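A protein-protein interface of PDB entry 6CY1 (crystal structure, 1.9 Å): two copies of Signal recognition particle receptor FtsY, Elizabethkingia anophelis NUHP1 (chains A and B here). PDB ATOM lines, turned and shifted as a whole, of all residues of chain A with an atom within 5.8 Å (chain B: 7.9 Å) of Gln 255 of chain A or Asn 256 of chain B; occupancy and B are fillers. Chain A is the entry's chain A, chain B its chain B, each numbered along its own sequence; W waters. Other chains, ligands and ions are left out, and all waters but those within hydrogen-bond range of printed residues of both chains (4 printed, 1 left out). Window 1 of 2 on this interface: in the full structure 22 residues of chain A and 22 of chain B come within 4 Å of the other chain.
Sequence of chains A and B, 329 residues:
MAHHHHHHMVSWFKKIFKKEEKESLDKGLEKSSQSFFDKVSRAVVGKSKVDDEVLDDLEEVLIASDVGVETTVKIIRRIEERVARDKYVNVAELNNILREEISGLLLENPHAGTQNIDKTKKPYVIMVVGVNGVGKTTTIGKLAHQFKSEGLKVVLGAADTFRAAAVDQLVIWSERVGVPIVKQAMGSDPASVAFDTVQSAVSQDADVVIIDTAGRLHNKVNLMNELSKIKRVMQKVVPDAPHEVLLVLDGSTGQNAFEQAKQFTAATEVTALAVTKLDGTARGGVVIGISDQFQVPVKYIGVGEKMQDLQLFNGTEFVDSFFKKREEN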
ATOM      1  N   ILE A  63     -20.982 -30.971  -4.806  1.00  0.00           N
ATOM      2  CA  ILE A  63     -20.379 -30.067  -5.788  1.00  0.00           C
ATOM      3  C   ILE A  63     -21.443 -29.536  -6.730  1.00  0.00           C
ATOM      4  O   ILE A  63     -21.498 -28.332  -7.020  1.00  0.00           O
ATOM      5  CB  ILE A  63     -19.241 -30.752  -6.563  1.00  0.00           C
ATOM      6  CG1 ILE A  63     -18.114 -31.127  -5.616  1.00  0.00           C
ATOM      7  CG2 ILE A  63     -18.723 -29.809  -7.660  1.00  0.00           C
ATOM      8  CD1 ILE A  63     -17.527 -29.953  -4.923  1.00  0.00           C
ATOM      9  N   ALA A  64     -22.295 -30.427  -7.241  1.00  0.00           N
ATOM     10  CA  ALA A  64     -23.354 -29.998  -8.161  1.00  0.00           C
ATOM     11  C   ALA A  64     -24.388 -29.108  -7.485  1.00  0.00           C
ATOM     12  O   ALA A  64     -25.217 -28.502  -8.182  1.00  0.00           O
ATOM     13  CB  ALA A  64     -24.052 -31.204  -8.778  1.00  0.00           C
ATOM     14  N   SER A  65     -24.366 -29.044  -6.156  1.00  0.00           N
ATOM     15  CA  SER A  65     -25.271 -28.237  -5.349  1.00  0.00           C
ATOM     16  C   SER A  65     -24.639 -26.916  -4.919  1.00  0.00           C
ATOM     17  O   SER A  65     -25.158 -26.251  -4.016  1.00  0.00           O
ATOM     18  CB  SER A  65     -25.715 -29.042  -4.121  1.00  0.00           C
ATOM     19  OG  SER A  65     -26.328 -30.273  -4.519  1.00  0.00           O
ATOM     20  N   ASP A  66     -23.518 -26.538  -5.531  1.00  0.00           N
ATOM     21  CA  ASP A  66     -22.841 -25.255  -5.316  1.00  0.00           C
ATOM     22  C   ASP A  66     -22.255 -25.114  -3.918  1.00  0.00           C
ATOM     23  O   ASP A  66     -21.962 -23.988  -3.493  1.00  0.00           O
ATOM     24  CB  ASP A  66     -23.766 -24.056  -5.580  1.00  0.00           C
ATOM     25  CG  ASP A  66     -24.030 -23.841  -7.066  1.00  0.00           C
ATOM     26  OD1 ASP A  66     -24.955 -24.487  -7.562  1.00  0.00           O
ATOM     27  OD2 ASP A  66     -23.317 -23.053  -7.732  1.00  0.00           O
ATOM     28  N   VAL A  67     -22.055 -26.226  -3.197  1.00  0.00           N
ATOM     29  CA  VAL A  67     -21.456 -26.129  -1.862  1.00  0.00           C
ATOM     30  C   VAL A  67     -19.980 -25.754  -1.950  1.00  0.00           C
ATOM     31  O   VAL A  67     -19.433 -25.101  -1.040  1.00  0.00           O
ATOM     32  CB  VAL A  67     -21.681 -27.443  -1.085  1.00  0.00           C
ATOM     33  CG1 VAL A  67     -20.926 -27.433   0.244  1.00  0.00           C
ATOM     34  CG2 VAL A  67     -23.188 -27.638  -0.833  1.00  0.00           C
ATOM     35  N   GLY A  68     -19.315 -26.128  -3.029  1.00  0.00           N
ATOM     36  CA  GLY A  68     -17.926 -25.741  -3.191  1.00  0.00           C
ATOM     37  C   GLY A  68     -16.991 -26.882  -2.833  1.00  0.00           C
ATOM     38  O   GLY A  68     -17.274 -27.691  -1.952  1.00  0.00           O
ATOM     39  N   VAL A  69     -15.839 -26.938  -3.507  1.00  0.00           N
ATOM     40  CA  VAL A  69     -14.948 -28.087  -3.348  1.00  0.00           C
ATOM     41  C   VAL A  69     -14.411 -28.182  -1.920  1.00  0.00           C
ATOM     42  O   VAL A  69     -14.462 -29.250  -1.299  1.00  0.00           O
ATOM     43  CB  VAL A  69     -13.799 -28.040  -4.366  1.00  0.00           C
ATOM     44  CG1 VAL A  69     -12.798 -29.190  -4.065  1.00  0.00           C
ATOM     45  CG2 VAL A  69     -14.341 -28.153  -5.778  1.00  0.00           C
ATOM     46  N   THR A 253     -26.797 -16.910  -8.063  1.00  0.00           N
ATOM     47  CA  THR A 253     -25.735 -17.303  -8.977  1.00  0.00           C
ATOM     48  C   THR A 253     -24.859 -18.408  -8.409  1.00  0.00           C
ATOM     49  O   THR A 253     -23.879 -18.784  -9.058  1.00  0.00           O
ATOM     50  CB  THR A 253     -24.864 -16.101  -9.367  1.00  0.00           C
ATOM     51  OG1 THR A 253     -24.137 -15.638  -8.221  1.00  0.00           O
ATOM     52  CG2 THR A 253     -25.727 -14.968  -9.930  1.00  0.00           C
ATOM     53  N   GLY A 254     -25.179 -18.927  -7.218  1.00  0.00           N
ATOM     54  CA  GLY A 254     -24.442 -20.086  -6.710  1.00  0.00           C
ATOM     55  C   GLY A 254     -22.991 -19.757  -6.447  1.00  0.00           C
ATOM     56  O   GLY A 254     -22.661 -18.679  -5.937  1.00  0.00           O
ATOM     57  N   GLN A 255     -22.090 -20.678  -6.822  1.00  0.00           N
ATOM     58  CA  GLN A 255     -20.677 -20.480  -6.497  1.00  0.00           C
ATOM     59  C   GLN A 255     -20.095 -19.227  -7.137  1.00  0.00           C
ATOM     60  O   GLN A 255     -19.020 -18.779  -6.720  1.00  0.00           O
ATOM     61  CB  GLN A 255     -19.845 -21.714  -6.883  1.00  0.00           C
ATOM     62  CG  GLN A 255     -19.800 -22.773  -5.767  1.00  0.00           C
ATOM     63  CD  GLN A 255     -18.938 -22.339  -4.568  1.00  0.00           C
ATOM     64  OE1 GLN A 255     -17.845 -21.799  -4.748  1.00  0.00           O
ATOM     65  NE2 GLN A 255     -19.439 -22.565  -3.341  1.00  0.00           N
ATOM     66  N   ASN A 256     -20.775 -18.642  -8.132  1.00  0.00           N
ATOM     67  CA  ASN A 256     -20.343 -17.345  -8.651  1.00  0.00           C
ATOM     68  C   ASN A 256     -20.331 -16.291  -7.552  1.00  0.00           C
ATOM     69  O   ASN A 256     -19.467 -15.404  -7.544  1.00  0.00           O
ATOM     70  CB  ASN A 256     -21.251 -16.913  -9.795  1.00  0.00           C
ATOM     71  CG  ASN A 256     -21.155 -17.847 -10.963  1.00  0.00           C
ATOM     72  OD1 ASN A 256     -20.137 -17.889 -11.647  1.00  0.00           O
ATOM     73  ND2 ASN A 256     -22.176 -18.670 -11.146  1.00  0.00           N
ATOM     74  N   ALA A 257     -21.283 -16.370  -6.617  1.00  0.00           N
ATOM     75  CA  ALA A 257     -21.293 -15.444  -5.486  1.00  0.00           C
ATOM     76  C   ALA A 257     -20.055 -15.633  -4.619  1.00  0.00           C
ATOM     77  O   ALA A 257     -19.485 -14.661  -4.100  1.00  0.00           O
ATOM     78  CB  ALA A 257     -22.554 -15.656  -4.650  1.00  0.00           C
ATOM     79  N   PHE A 258     -19.629 -16.884  -4.458  1.00  0.00           N
ATOM     80  CA  PHE A 258     -18.411 -17.192  -3.723  1.00  0.00           C
ATOM     81  C   PHE A 258     -17.215 -16.514  -4.384  1.00  0.00           C
ATOM     82  O   PHE A 258     -16.407 -15.846  -3.723  1.00  0.00           O
ATOM     83  CB  PHE A 258     -18.249 -18.719  -3.689  1.00  0.00           C
ATOM     84  CG  PHE A 258     -17.191 -19.230  -2.764  1.00  0.00           C
ATOM     85  CD1 PHE A 258     -15.845 -19.099  -3.072  1.00  0.00           C
ATOM     86  CD2 PHE A 258     -17.551 -19.950  -1.629  1.00  0.00           C
ATOM     87  CE1 PHE A 258     -14.866 -19.615  -2.230  1.00  0.00           C
ATOM     88  CE2 PHE A 258     -16.574 -20.465  -0.780  1.00  0.00           C
ATOM     89  CZ  PHE A 258     -15.232 -20.301  -1.084  1.00  0.00           C
ATOM     90  N   GLU A 259     -17.109 -16.644  -5.708  1.00  0.00           N
ATOM     91  CA  GLU A 259     -15.986 -16.031  -6.418  1.00  0.00           C
ATOM     92  C   GLU A 259     -16.065 -14.510  -6.377  1.00  0.00           C
ATOM     93  O   GLU A 259     -15.037 -13.824  -6.288  1.00  0.00           O
ATOM     94  CB  GLU A 259     -15.988 -16.512  -7.874  1.00  0.00           C
ATOM     95  CG  GLU A 259     -14.734 -16.219  -8.694  1.00  0.00           C
ATOM     96  CD  GLU A 259     -13.477 -16.850  -8.135  1.00  0.00           C
ATOM     97  OE1 GLU A 259     -12.409 -16.206  -8.234  1.00  0.00           O
ATOM     98  OE2 GLU A 259     -13.554 -17.986  -7.614  1.00  0.00           O
ATOM     99  N   GLN A 260     -17.273 -13.966  -6.483  1.00  0.00           N
ATOM    100  CA  GLN A 260     -17.425 -12.518  -6.421  1.00  0.00           C
ATOM    101  C   GLN A 260     -17.032 -11.987  -5.048  1.00  0.00           C
ATOM    102  O   GLN A 260     -16.425 -10.917  -4.940  1.00  0.00           O
ATOM    103  CB  GLN A 260     -18.857 -12.142  -6.788  1.00  0.00           C
ATOM    104  CG  GLN A 260     -19.103 -10.673  -6.953  1.00  0.00           C
ATOM    105  CD  GLN A 260     -20.496 -10.409  -7.475  1.00  0.00           C
ATOM    106  OE1 GLN A 260     -21.436 -10.201  -6.705  1.00  0.00           O
ATOM    107  NE2 GLN A 260     -20.642 -10.438  -8.798  1.00  0.00           N
ATOM    108  N   ARG A 283     -29.536 -23.172  -6.124  1.00  0.00           N
ATOM    109  CA  ARG A 283     -28.112 -23.074  -5.845  1.00  0.00           C
ATOM    110  C   ARG A 283     -27.819 -22.539  -4.446  1.00  0.00           C
ATOM    111  O   ARG A 283     -26.699 -22.089  -4.180  1.00  0.00           O
ATOM    112  CB  ARG A 283     -27.467 -22.177  -6.903  1.00  0.00           C
ATOM    113  CG  ARG A 283     -27.827 -22.615  -8.320  1.00  0.00           C
ATOM    114  CD  ARG A 283     -27.169 -21.724  -9.343  1.00  0.00           C
ATOM    115  NE  ARG A 283     -25.791 -22.123  -9.605  1.00  0.00           N
ATOM    116  CZ  ARG A 283     -25.107 -21.715 -10.669  1.00  0.00           C
ATOM    117  NH1 ARG A 283     -25.699 -20.892 -11.533  1.00  0.00           N
ATOM    118  NH2 ARG A 283     -23.850 -22.125 -10.868  1.00  0.00           N
ATOM    119  N   GLY A 285     -27.156 -23.852  -1.736  1.00  0.00           N
ATOM    120  CA  GLY A 285     -26.082 -24.489  -0.998  1.00  0.00           C
ATOM    121  C   GLY A 285     -24.807 -23.674  -0.962  1.00  0.00           C
ATOM    122  O   GLY A 285     -23.939 -23.936  -0.125  1.00  0.00           O
ATOM    123  N   VAL A 286     -24.683 -22.666  -1.834  1.00  0.00           N
ATOM    124  CA  VAL A 286     -23.495 -21.818  -1.780  1.00  0.00           C
ATOM    125  C   VAL A 286     -23.358 -21.161  -0.406  1.00  0.00           C
ATOM    126  O   VAL A 286     -22.240 -20.846   0.031  1.00  0.00           O
ATOM    127  CB  VAL A 286     -23.508 -20.762  -2.909  1.00  0.00           C
ATOM    128  CG1 VAL A 286     -24.634 -19.724  -2.678  1.00  0.00           C
ATOM    129  CG2 VAL A 286     -22.153 -20.093  -2.999  1.00  0.00           C
ATOM    130  N   GLY A 289     -21.074 -23.215   1.779  1.00  0.00           N
ATOM    131  CA  GLY A 289     -19.669 -23.036   1.438  1.00  0.00           C
ATOM    132  C   GLY A 289     -19.136 -21.674   1.847  1.00  0.00           C
ATOM    133  O   GLY A 289     -18.005 -21.559   2.326  1.00  0.00           O
ATOM    134  N   ILE A 290     -19.936 -20.628   1.662  1.00  0.00           N
ATOM    135  CA  ILE A 290     -19.493 -19.290   2.072  1.00  0.00           C
ATOM    136  C   ILE A 290     -19.282 -19.238   3.578  1.00  0.00           C
ATOM    137  O   ILE A 290     -18.229 -18.795   4.065  1.00  0.00           O
ATOM    138  CB  ILE A 290     -20.505 -18.238   1.602  1.00  0.00           C
ATOM    139  CG1 ILE A 290     -20.448 -18.129   0.079  1.00  0.00           C
ATOM    140  CG2 ILE A 290     -20.228 -16.886   2.283  1.00  0.00           C
ATOM    141  CD1 ILE A 290     -21.461 -17.176  -0.503  1.00  0.00           C
ATOM    142  N   ILE B  63     -22.650 -12.802 -15.434  1.00  0.00           N
ATOM    143  CA  ILE B  63     -22.361 -13.512 -14.187  1.00  0.00           C
ATOM    144  C   ILE B  63     -23.443 -14.549 -13.927  1.00  0.00           C
ATOM    145  O   ILE B  63     -23.155 -15.722 -13.668  1.00  0.00           O
ATOM    146  CB  ILE B  63     -22.242 -12.524 -13.010  1.00  0.00           C
ATOM    147  CG1 ILE B  63     -21.067 -11.561 -13.207  1.00  0.00           C
ATOM    148  CG2 ILE B  63     -22.096 -13.276 -11.686  1.00  0.00           C
ATOM    149  CD1 ILE B  63     -19.730 -12.253 -13.291  1.00  0.00           C
ATOM    150  N   ASP B  66     -23.231 -17.963 -15.686  1.00  0.00           N
ATOM    151  CA  ASP B  66     -22.081 -18.813 -15.382  1.00  0.00           C
ATOM    152  C   ASP B  66     -20.891 -18.590 -16.304  1.00  0.00           C
ATOM    153  O   ASP B  66     -20.019 -19.465 -16.409  1.00  0.00           O
ATOM    154  CB  ASP B  66     -22.461 -20.293 -15.380  1.00  0.00           C
ATOM    155  CG  ASP B  66     -23.145 -20.698 -14.114  1.00  0.00           C
ATOM    156  OD1 ASP B  66     -24.378 -20.530 -14.013  1.00  0.00           O
ATOM    157  OD2 ASP B  66     -22.429 -21.159 -13.200  1.00  0.00           O
ATOM    158  N   VAL B  69     -16.586 -14.741 -13.285  1.00  0.00           N
ATOM    159  CA  VAL B  69     -16.310 -13.358 -12.895  1.00  0.00           C
ATOM    160  C   VAL B  69     -15.132 -12.795 -13.680  1.00  0.00           C
ATOM    161  O   VAL B  69     -15.237 -11.736 -14.309  1.00  0.00           O
ATOM    162  CB  VAL B  69     -16.070 -13.261 -11.380  1.00  0.00           C
ATOM    163  CG1 VAL B  69     -15.660 -11.847 -11.019  1.00  0.00           C
ATOM    164  CG2 VAL B  69     -17.319 -13.681 -10.622  1.00  0.00           C
ATOM    165  N   LEU B 249     -15.731 -33.046 -17.438  1.00  0.00           N
ATOM    166  CA  LEU B 249     -16.393 -32.099 -16.550  1.00  0.00           C
ATOM    167  C   LEU B 249     -17.876 -32.028 -16.886  1.00  0.00           C
ATOM    168  O   LEU B 249     -18.269 -32.142 -18.046  1.00  0.00           O
ATOM    169  CB  LEU B 249     -15.770 -30.700 -16.678  1.00  0.00           C
ATOM    170  CG  LEU B 249     -14.255 -30.684 -16.449  1.00  0.00           C
ATOM    171  CD1 LEU B 249     -13.632 -29.350 -16.899  1.00  0.00           C
ATOM    172  CD2 LEU B 249     -13.946 -31.000 -15.001  1.00  0.00           C
ATOM    173  N   ASP B 250     -18.698 -31.786 -15.871  1.00  0.00           N
ATOM    174  CA  ASP B 250     -20.150 -31.707 -16.064  1.00  0.00           C
ATOM    175  C   ASP B 250     -20.542 -30.249 -16.289  1.00  0.00           C
ATOM    176  O   ASP B 250     -20.619 -29.458 -15.348  1.00  0.00           O
ATOM    177  CB  ASP B 250     -20.875 -32.314 -14.863  1.00  0.00           C
ATOM    178  CG  ASP B 250     -22.376 -32.422 -15.071  1.00  0.00           C
ATOM    179  OD1 ASP B 250     -22.910 -31.762 -15.985  1.00  0.00           O
ATOM    180  OD2 ASP B 250     -23.020 -33.195 -14.330  1.00  0.00           O
ATOM    181  N   GLY B 251     -20.819 -29.887 -17.541  1.00  0.00           N
ATOM    182  CA  GLY B 251     -21.182 -28.512 -17.815  1.00  0.00           C
ATOM    183  C   GLY B 251     -22.533 -28.109 -17.263  1.00  0.00           C
ATOM    184  O   GLY B 251     -22.806 -26.912 -17.135  1.00  0.00           O
ATOM    185  N   SER B 252     -23.376 -29.077 -16.911  1.00  0.00           N
ATOM    186  CA  SER B 252     -24.662 -28.713 -16.337  1.00  0.00           C
ATOM    187  C   SER B 252     -24.532 -28.127 -14.942  1.00  0.00           C
ATOM    188  O   SER B 252     -25.510 -27.569 -14.437  1.00  0.00           O
ATOM    189  CB  SER B 252     -25.603 -29.923 -16.312  1.00  0.00           C
ATOM    190  OG  SER B 252     -25.315 -30.804 -15.246  1.00  0.00           O
ATOM    191  N   THR B 253     -23.360 -28.210 -14.319  1.00  0.00           N
ATOM    192  CA  THR B 253     -23.152 -27.561 -13.026  1.00  0.00           C
ATOM    193  C   THR B 253     -22.554 -26.173 -13.165  1.00  0.00           C
ATOM    194  O   THR B 253     -22.350 -25.495 -12.144  1.00  0.00           O
ATOM    195  CB  THR B 253     -22.249 -28.422 -12.114  1.00  0.00           C
ATOM    196  OG1 THR B 253     -20.931 -28.535 -12.683  1.00  0.00           O
ATOM    197  CG2 THR B 253     -22.839 -29.811 -11.906  1.00  0.00           C
ATOM    198  N   GLY B 254     -22.310 -25.714 -14.393  1.00  0.00           N
ATOM    199  CA  GLY B 254     -21.833 -24.354 -14.559  1.00  0.00           C
ATOM    200  C   GLY B 254     -20.466 -24.168 -13.936  1.00  0.00           C
ATOM    201  O   GLY B 254     -19.584 -25.029 -14.039  1.00  0.00           O
ATOM    202  N   GLN B 255     -20.288 -23.037 -13.253  1.00  0.00           N
ATOM    203  CA  GLN B 255     -18.982 -22.701 -12.706  1.00  0.00           C
ATOM    204  C   GLN B 255     -18.505 -23.699 -11.646  1.00  0.00           C
ATOM    205  O   GLN B 255     -17.320 -23.686 -11.296  1.00  0.00           O
ATOM    206  CB  GLN B 255     -19.017 -21.282 -12.128  1.00  0.00           C
ATOM    207  CG  GLN B 255     -18.863 -20.188 -13.204  1.00  0.00           C
ATOM    208  CD  GLN B 255     -17.470 -20.121 -13.817  1.00  0.00           C
ATOM    209  OE1 GLN B 255     -16.467 -20.240 -13.112  1.00  0.00           O
ATOM    210  NE2 GLN B 255     -17.405 -19.900 -15.143  1.00  0.00           N
ATOM    211  N   ASN B 256     -19.387 -24.551 -11.113  1.00  0.00           N
ATOM    212  CA  ASN B 256     -18.908 -25.594 -10.205  1.00  0.00           C
ATOM    213  C   ASN B 256     -17.897 -26.489 -10.903  1.00  0.00           C
ATOM    214  O   ASN B 256     -16.912 -26.929 -10.298  1.00  0.00           O
ATOM    215  CB  ASN B 256     -20.081 -26.411  -9.667  1.00  0.00           C
ATOM    216  CG  ASN B 256     -21.031 -25.577  -8.847  1.00  0.00           C
ATOM    217  OD1 ASN B 256     -20.684 -25.110  -7.761  1.00  0.00           O
ATOM    218  ND2 ASN B 256     -22.241 -25.386  -9.352  1.00  0.00           N
ATOM    219  N   ALA B 257     -18.116 -26.745 -12.192  1.00  0.00           N
ATOM    220  CA  ALA B 257     -17.175 -27.546 -12.973  1.00  0.00           C
ATOM    221  C   ALA B 257     -15.825 -26.861 -13.108  1.00  0.00           C
ATOM    222  O   ALA B 257     -14.790 -27.531 -13.192  1.00  0.00           O
ATOM    223  CB  ALA B 257     -17.761 -27.825 -14.355  1.00  0.00           C
ATOM    224  N   PHE B 258     -15.832 -25.529 -13.198  1.00  0.00           N
ATOM    225  CA  PHE B 258     -14.600 -24.753 -13.301  1.00  0.00           C
ATOM    226  C   PHE B 258     -13.721 -24.951 -12.076  1.00  0.00           C
ATOM    227  O   PHE B 258     -12.519 -25.212 -12.192  1.00  0.00           O
ATOM    228  CB  PHE B 258     -14.974 -23.276 -13.486  1.00  0.00           C
ATOM    229  CG  PHE B 258     -13.822 -22.352 -13.761  1.00  0.00           C
ATOM    230  CD1 PHE B 258     -12.963 -21.967 -12.745  1.00  0.00           C
ATOM    231  CD2 PHE B 258     -13.650 -21.798 -15.016  1.00  0.00           C
ATOM    232  CE1 PHE B 258     -11.923 -21.096 -12.984  1.00  0.00           C
ATOM    233  CE2 PHE B 258     -12.607 -20.922 -15.264  1.00  0.00           C
ATOM    234  CZ  PHE B 258     -11.746 -20.567 -14.242  1.00  0.00           C
ATOM    235  N   GLU B 259     -14.298 -24.802 -10.888  1.00  0.00           N
ATOM    236  CA  GLU B 259     -13.495 -24.923  -9.681  1.00  0.00           C
ATOM    237  C   GLU B 259     -13.085 -26.376  -9.459  1.00  0.00           C
ATOM    238  O   GLU B 259     -11.986 -26.654  -8.962  1.00  0.00           O
ATOM    239  CB  GLU B 259     -14.260 -24.355  -8.488  1.00  0.00           C
ATOM    240  CG  GLU B 259     -13.350 -23.949  -7.347  1.00  0.00           C
ATOM    241  CD  GLU B 259     -12.359 -22.869  -7.763  1.00  0.00           C
ATOM    242  OE1 GLU B 259     -11.197 -22.923  -7.308  1.00  0.00           O
ATOM    243  OE2 GLU B 259     -12.741 -21.973  -8.553  1.00  0.00           O
ATOM    244  N   GLN B 260     -13.963 -27.317  -9.812  1.00  0.00           N
ATOM    245  CA  GLN B 260     -13.596 -28.727  -9.740  1.00  0.00           C
ATOM    246  C   GLN B 260     -12.429 -29.028 -10.671  1.00  0.00           C
ATOM    247  O   GLN B 260     -11.501 -29.759 -10.305  1.00  0.00           O
ATOM    248  CB  GLN B 260     -14.796 -29.605 -10.113  1.00  0.00           C
ATOM    249  CG  GLN B 260     -14.520 -31.096  -9.997  1.00  0.00           C
ATOM    250  CD  GLN B 260     -15.717 -31.950 -10.363  1.00  0.00           C
ATOM    251  OE1 GLN B 260     -15.882 -32.332 -11.525  1.00  0.00           O
ATOM    252  NE2 GLN B 260     -16.531 -32.293  -9.377  1.00  0.00           N
ATOM    253  N   ALA B 261     -12.443 -28.444 -11.869  1.00  0.00           N
ATOM    254  CA  ALA B 261     -11.351 -28.652 -12.816  1.00  0.00           C
ATOM    255  C   ALA B 261     -10.051 -28.032 -12.316  1.00  0.00           C
ATOM    256  O   ALA B 261      -8.968 -28.587 -12.533  1.00  0.00           O
ATOM    257  CB  ALA B 261     -11.721 -28.066 -14.172  1.00  0.00           C
ATOM    258  N   LYS B 262     -10.143 -26.869 -11.670  1.00  0.00           N
ATOM    259  CA  LYS B 262      -8.976 -26.251 -11.050  1.00  0.00           C
ATOM    260  C   LYS B 262      -8.280 -27.216 -10.091  1.00  0.00           C
ATOM    261  O   LYS B 262      -7.048 -27.256 -10.033  1.00  0.00           O
ATOM    262  CB  LYS B 262      -9.407 -24.973 -10.333  1.00  0.00           C
ATOM    263  CG  LYS B 262      -8.497 -23.772 -10.525  1.00  0.00           C
ATOM    264  CD  LYS B 262      -9.057 -22.559  -9.785  1.00  0.00           C
ATOM    265  CE  LYS B 262      -8.168 -21.333  -9.924  1.00  0.00           C
ATOM    266  NZ  LYS B 262      -8.756 -20.147  -9.225  1.00  0.00           N
ATOM    267  N   ARG B 283     -26.516 -23.349 -18.092  1.00  0.00           N
ATOM    268  CA  ARG B 283     -25.231 -22.865 -17.588  1.00  0.00           C
ATOM    269  C   ARG B 283     -24.074 -23.083 -18.561  1.00  0.00           C
ATOM    270  O   ARG B 283     -22.911 -23.021 -18.147  1.00  0.00           O
ATOM    271  CB  ARG B 283     -24.912 -23.524 -16.241  1.00  0.00           C
ATOM    272  CG  ARG B 283     -26.032 -23.347 -15.215  1.00  0.00           C
ATOM    273  CD  ARG B 283     -25.653 -23.976 -13.880  1.00  0.00           C
ATOM    274  NE  ARG B 283     -26.812 -24.148 -13.014  1.00  0.00           N
ATOM    275  CZ  ARG B 283     -26.755 -24.756 -11.834  1.00  0.00           C
ATOM    276  NH1 ARG B 283     -25.592 -25.223 -11.398  1.00  0.00           N
ATOM    277  NH2 ARG B 283     -27.847 -24.898 -11.098  1.00  0.00           N
ATOM    278  N   VAL B 286     -20.287 -21.555 -19.011  1.00  0.00           N
ATOM    279  CA  VAL B 286     -19.067 -21.944 -18.300  1.00  0.00           C
ATOM    280  C   VAL B 286     -17.969 -22.357 -19.274  1.00  0.00           C
ATOM    281  O   VAL B 286     -16.776 -22.205 -18.981  1.00  0.00           O
ATOM    282  CB  VAL B 286     -19.367 -23.072 -17.283  1.00  0.00           C
ATOM    283  CG1 VAL B 286     -19.804 -24.332 -17.978  1.00  0.00           C
ATOM    284  CG2 VAL B 286     -18.135 -23.362 -16.437  1.00  0.00           C
ATOM    285  N   ILE B 290     -14.116 -21.294 -19.038  1.00  0.00           N
ATOM    286  CA  ILE B 290     -13.063 -22.309 -18.986  1.00  0.00           C
ATOM    287  C   ILE B 290     -12.065 -22.098 -20.116  1.00  0.00           C
ATOM    288  O   ILE B 290     -10.848 -22.077 -19.897  1.00  0.00           O
ATOM    289  CB  ILE B 290     -13.657 -23.725 -19.024  1.00  0.00           C
ATOM    290  CG1 ILE B 290     -14.389 -24.035 -17.718  1.00  0.00           C
ATOM    291  CG2 ILE B 290     -12.544 -24.749 -19.264  1.00  0.00           C
ATOM    292  CD1 ILE B 290     -15.057 -25.407 -17.724  1.00  0.00           C
HETATM  293  O   HOH W   1     -11.334 -19.005  -9.750  1.00  0.00           O
HETATM  294  O   HOH W   2     -17.329 -16.800 -11.333  1.00  0.00           O
HETATM  295  O   HOH W   3     -20.697 -16.353 -13.694  1.00  0.00           O
HETATM  296  O   HOH W   4     -19.698 -26.581  -5.800  1.00  0.00           O
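OD1 of Asp 66 of chain A lies within salt-bridge range of NH1 of Arg 283 of chain B. The guanidinium group (NH1) of Arg 283 of chain A is in salt-bridge range of the side-chain carboxylate (OD1) of Asp 66 of chain B. OD2 of Asp 66 of chain A lies within hydrogen-bond range of ND2 of Asn 256 of chain B (3.0 Å). The side-chain carboxylate (OD2) of Asp 66 of chain B lies within hydrogen-bond range of the side-chain amide nitrogen (ND2) of Asn 256 of chain A, 3.2 Å away. The side-chain amide oxygen (OD1) of Asn 256 of chain B sits close to the backbone carbonyl oxygen (O) of Ile 63 of chain A, 3.4 Å away.
NH1 of Arg 283 of chain B sits at hydrogen-bond distance from O of Thr 253 of chain B (3.3 Å). The side-chain carboxylate of Asp 66 of chain A lies within salt-bridge range of the guanidinium group of Arg 283 of chain A (3.2 Å). The backbone carbonyl oxygen (O) of Thr 253 of chain A lies within hydrogen-bond range of the side-chain amide nitrogen (ND2) of Asn 256 of chain A (2.7 Å).
CG2 of Ile 63 of chain A touches NE2 of Gln 260 of chain B (3.7 Å). Ala 64 of chain A touches Thr 253 of chain B (CB to CG2, 3.6 Å). Asn 256 of chain B touches Gln 255 of chain A (OD1 to CG, 3.2 Å). CG of Asn 256 of chain A touches O of Ile 63 of chain B, 3.98 Å away. Asn 256 of chain A touches Gln 255 of chain B. Thr 253 of chain B touches Arg 283 of chain A (O to NH2, 3.9 Å). NE of Arg 283 of chain A touches CZ of Arg 283 of chain B (3.6 Å).
Gln 255 of chain A touches one residue of chain B. No residue of chain B comes within 4 Å of Gly 254 of chain A. Of the printed residues of chain A, Thr 253 of chain B touches Ala 64 (3.6 Å) and Arg 283 (3.9 Å). Printed residues of chain B within 4 Å of Asp 66 of chain A: Asn 256 and Arg 283. The nearest printed residue of chain B that does not touch Asn 256 of chain A is Val 69 of chain B (4.1 Å).
Of the 20 printed residues of chain B, 7 touch a printed residue of chain A. Printed residues of chain A that touch a printed residue of chain B: Ile 63, Ala 64, Asp 66, Gln 255, Asn 256 and Arg 283. Hydrophobic or aromatic side chains of chain A that line the printed part of chain B: Ile 63 and Ala 64. Among the printed residues, 13 pairs touch across the chains. Among the printed residues, Asp or Glu carboxylates within 4 Å of a Lys or Arg side-chain nitrogen of the other chain: Asp 66 of chain A with Arg 283 of chain B (3.96 Å) and Arg 283 of chain A with Asp 66 of chain B (2.8 Å).
Ile 63 of chain A touches Asn 256 of chain B, and with the chains exchanged Asn 256 of chain A touches Ile 63 of chain B. Ile 63 of chain A touches Gln 260 of chain B, but with the chains exchanged Gln 260 of chain A does not touch Ile 63 of chain B (4.3 Å). Asp 66 of chain A touches Asn 256 of chain B, and with the chains exchanged Asn 256 of chain A touches Asp 66 of chain B.
Water W3 lies within hydrogen-bond range of the backbone carbonyl oxygen of Ile 63 of chain B and the side-chain amide oxygen of Asn 256 of chain A. Water W4 lies within hydrogen-bond range of the side-chain amide oxygen (OD1) of Asn 256 of chain B (2.6 Å), the backbone carbonyl oxygen (O) of Ile 63 of chain A (2.8 Å) and the backbone NH (N) of Gly 68 of chain A (2.8 Å). Water W2 lies within hydrogen-bond range of N of Val 69 of chain B and OD1 of Asn 256 of chain A.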
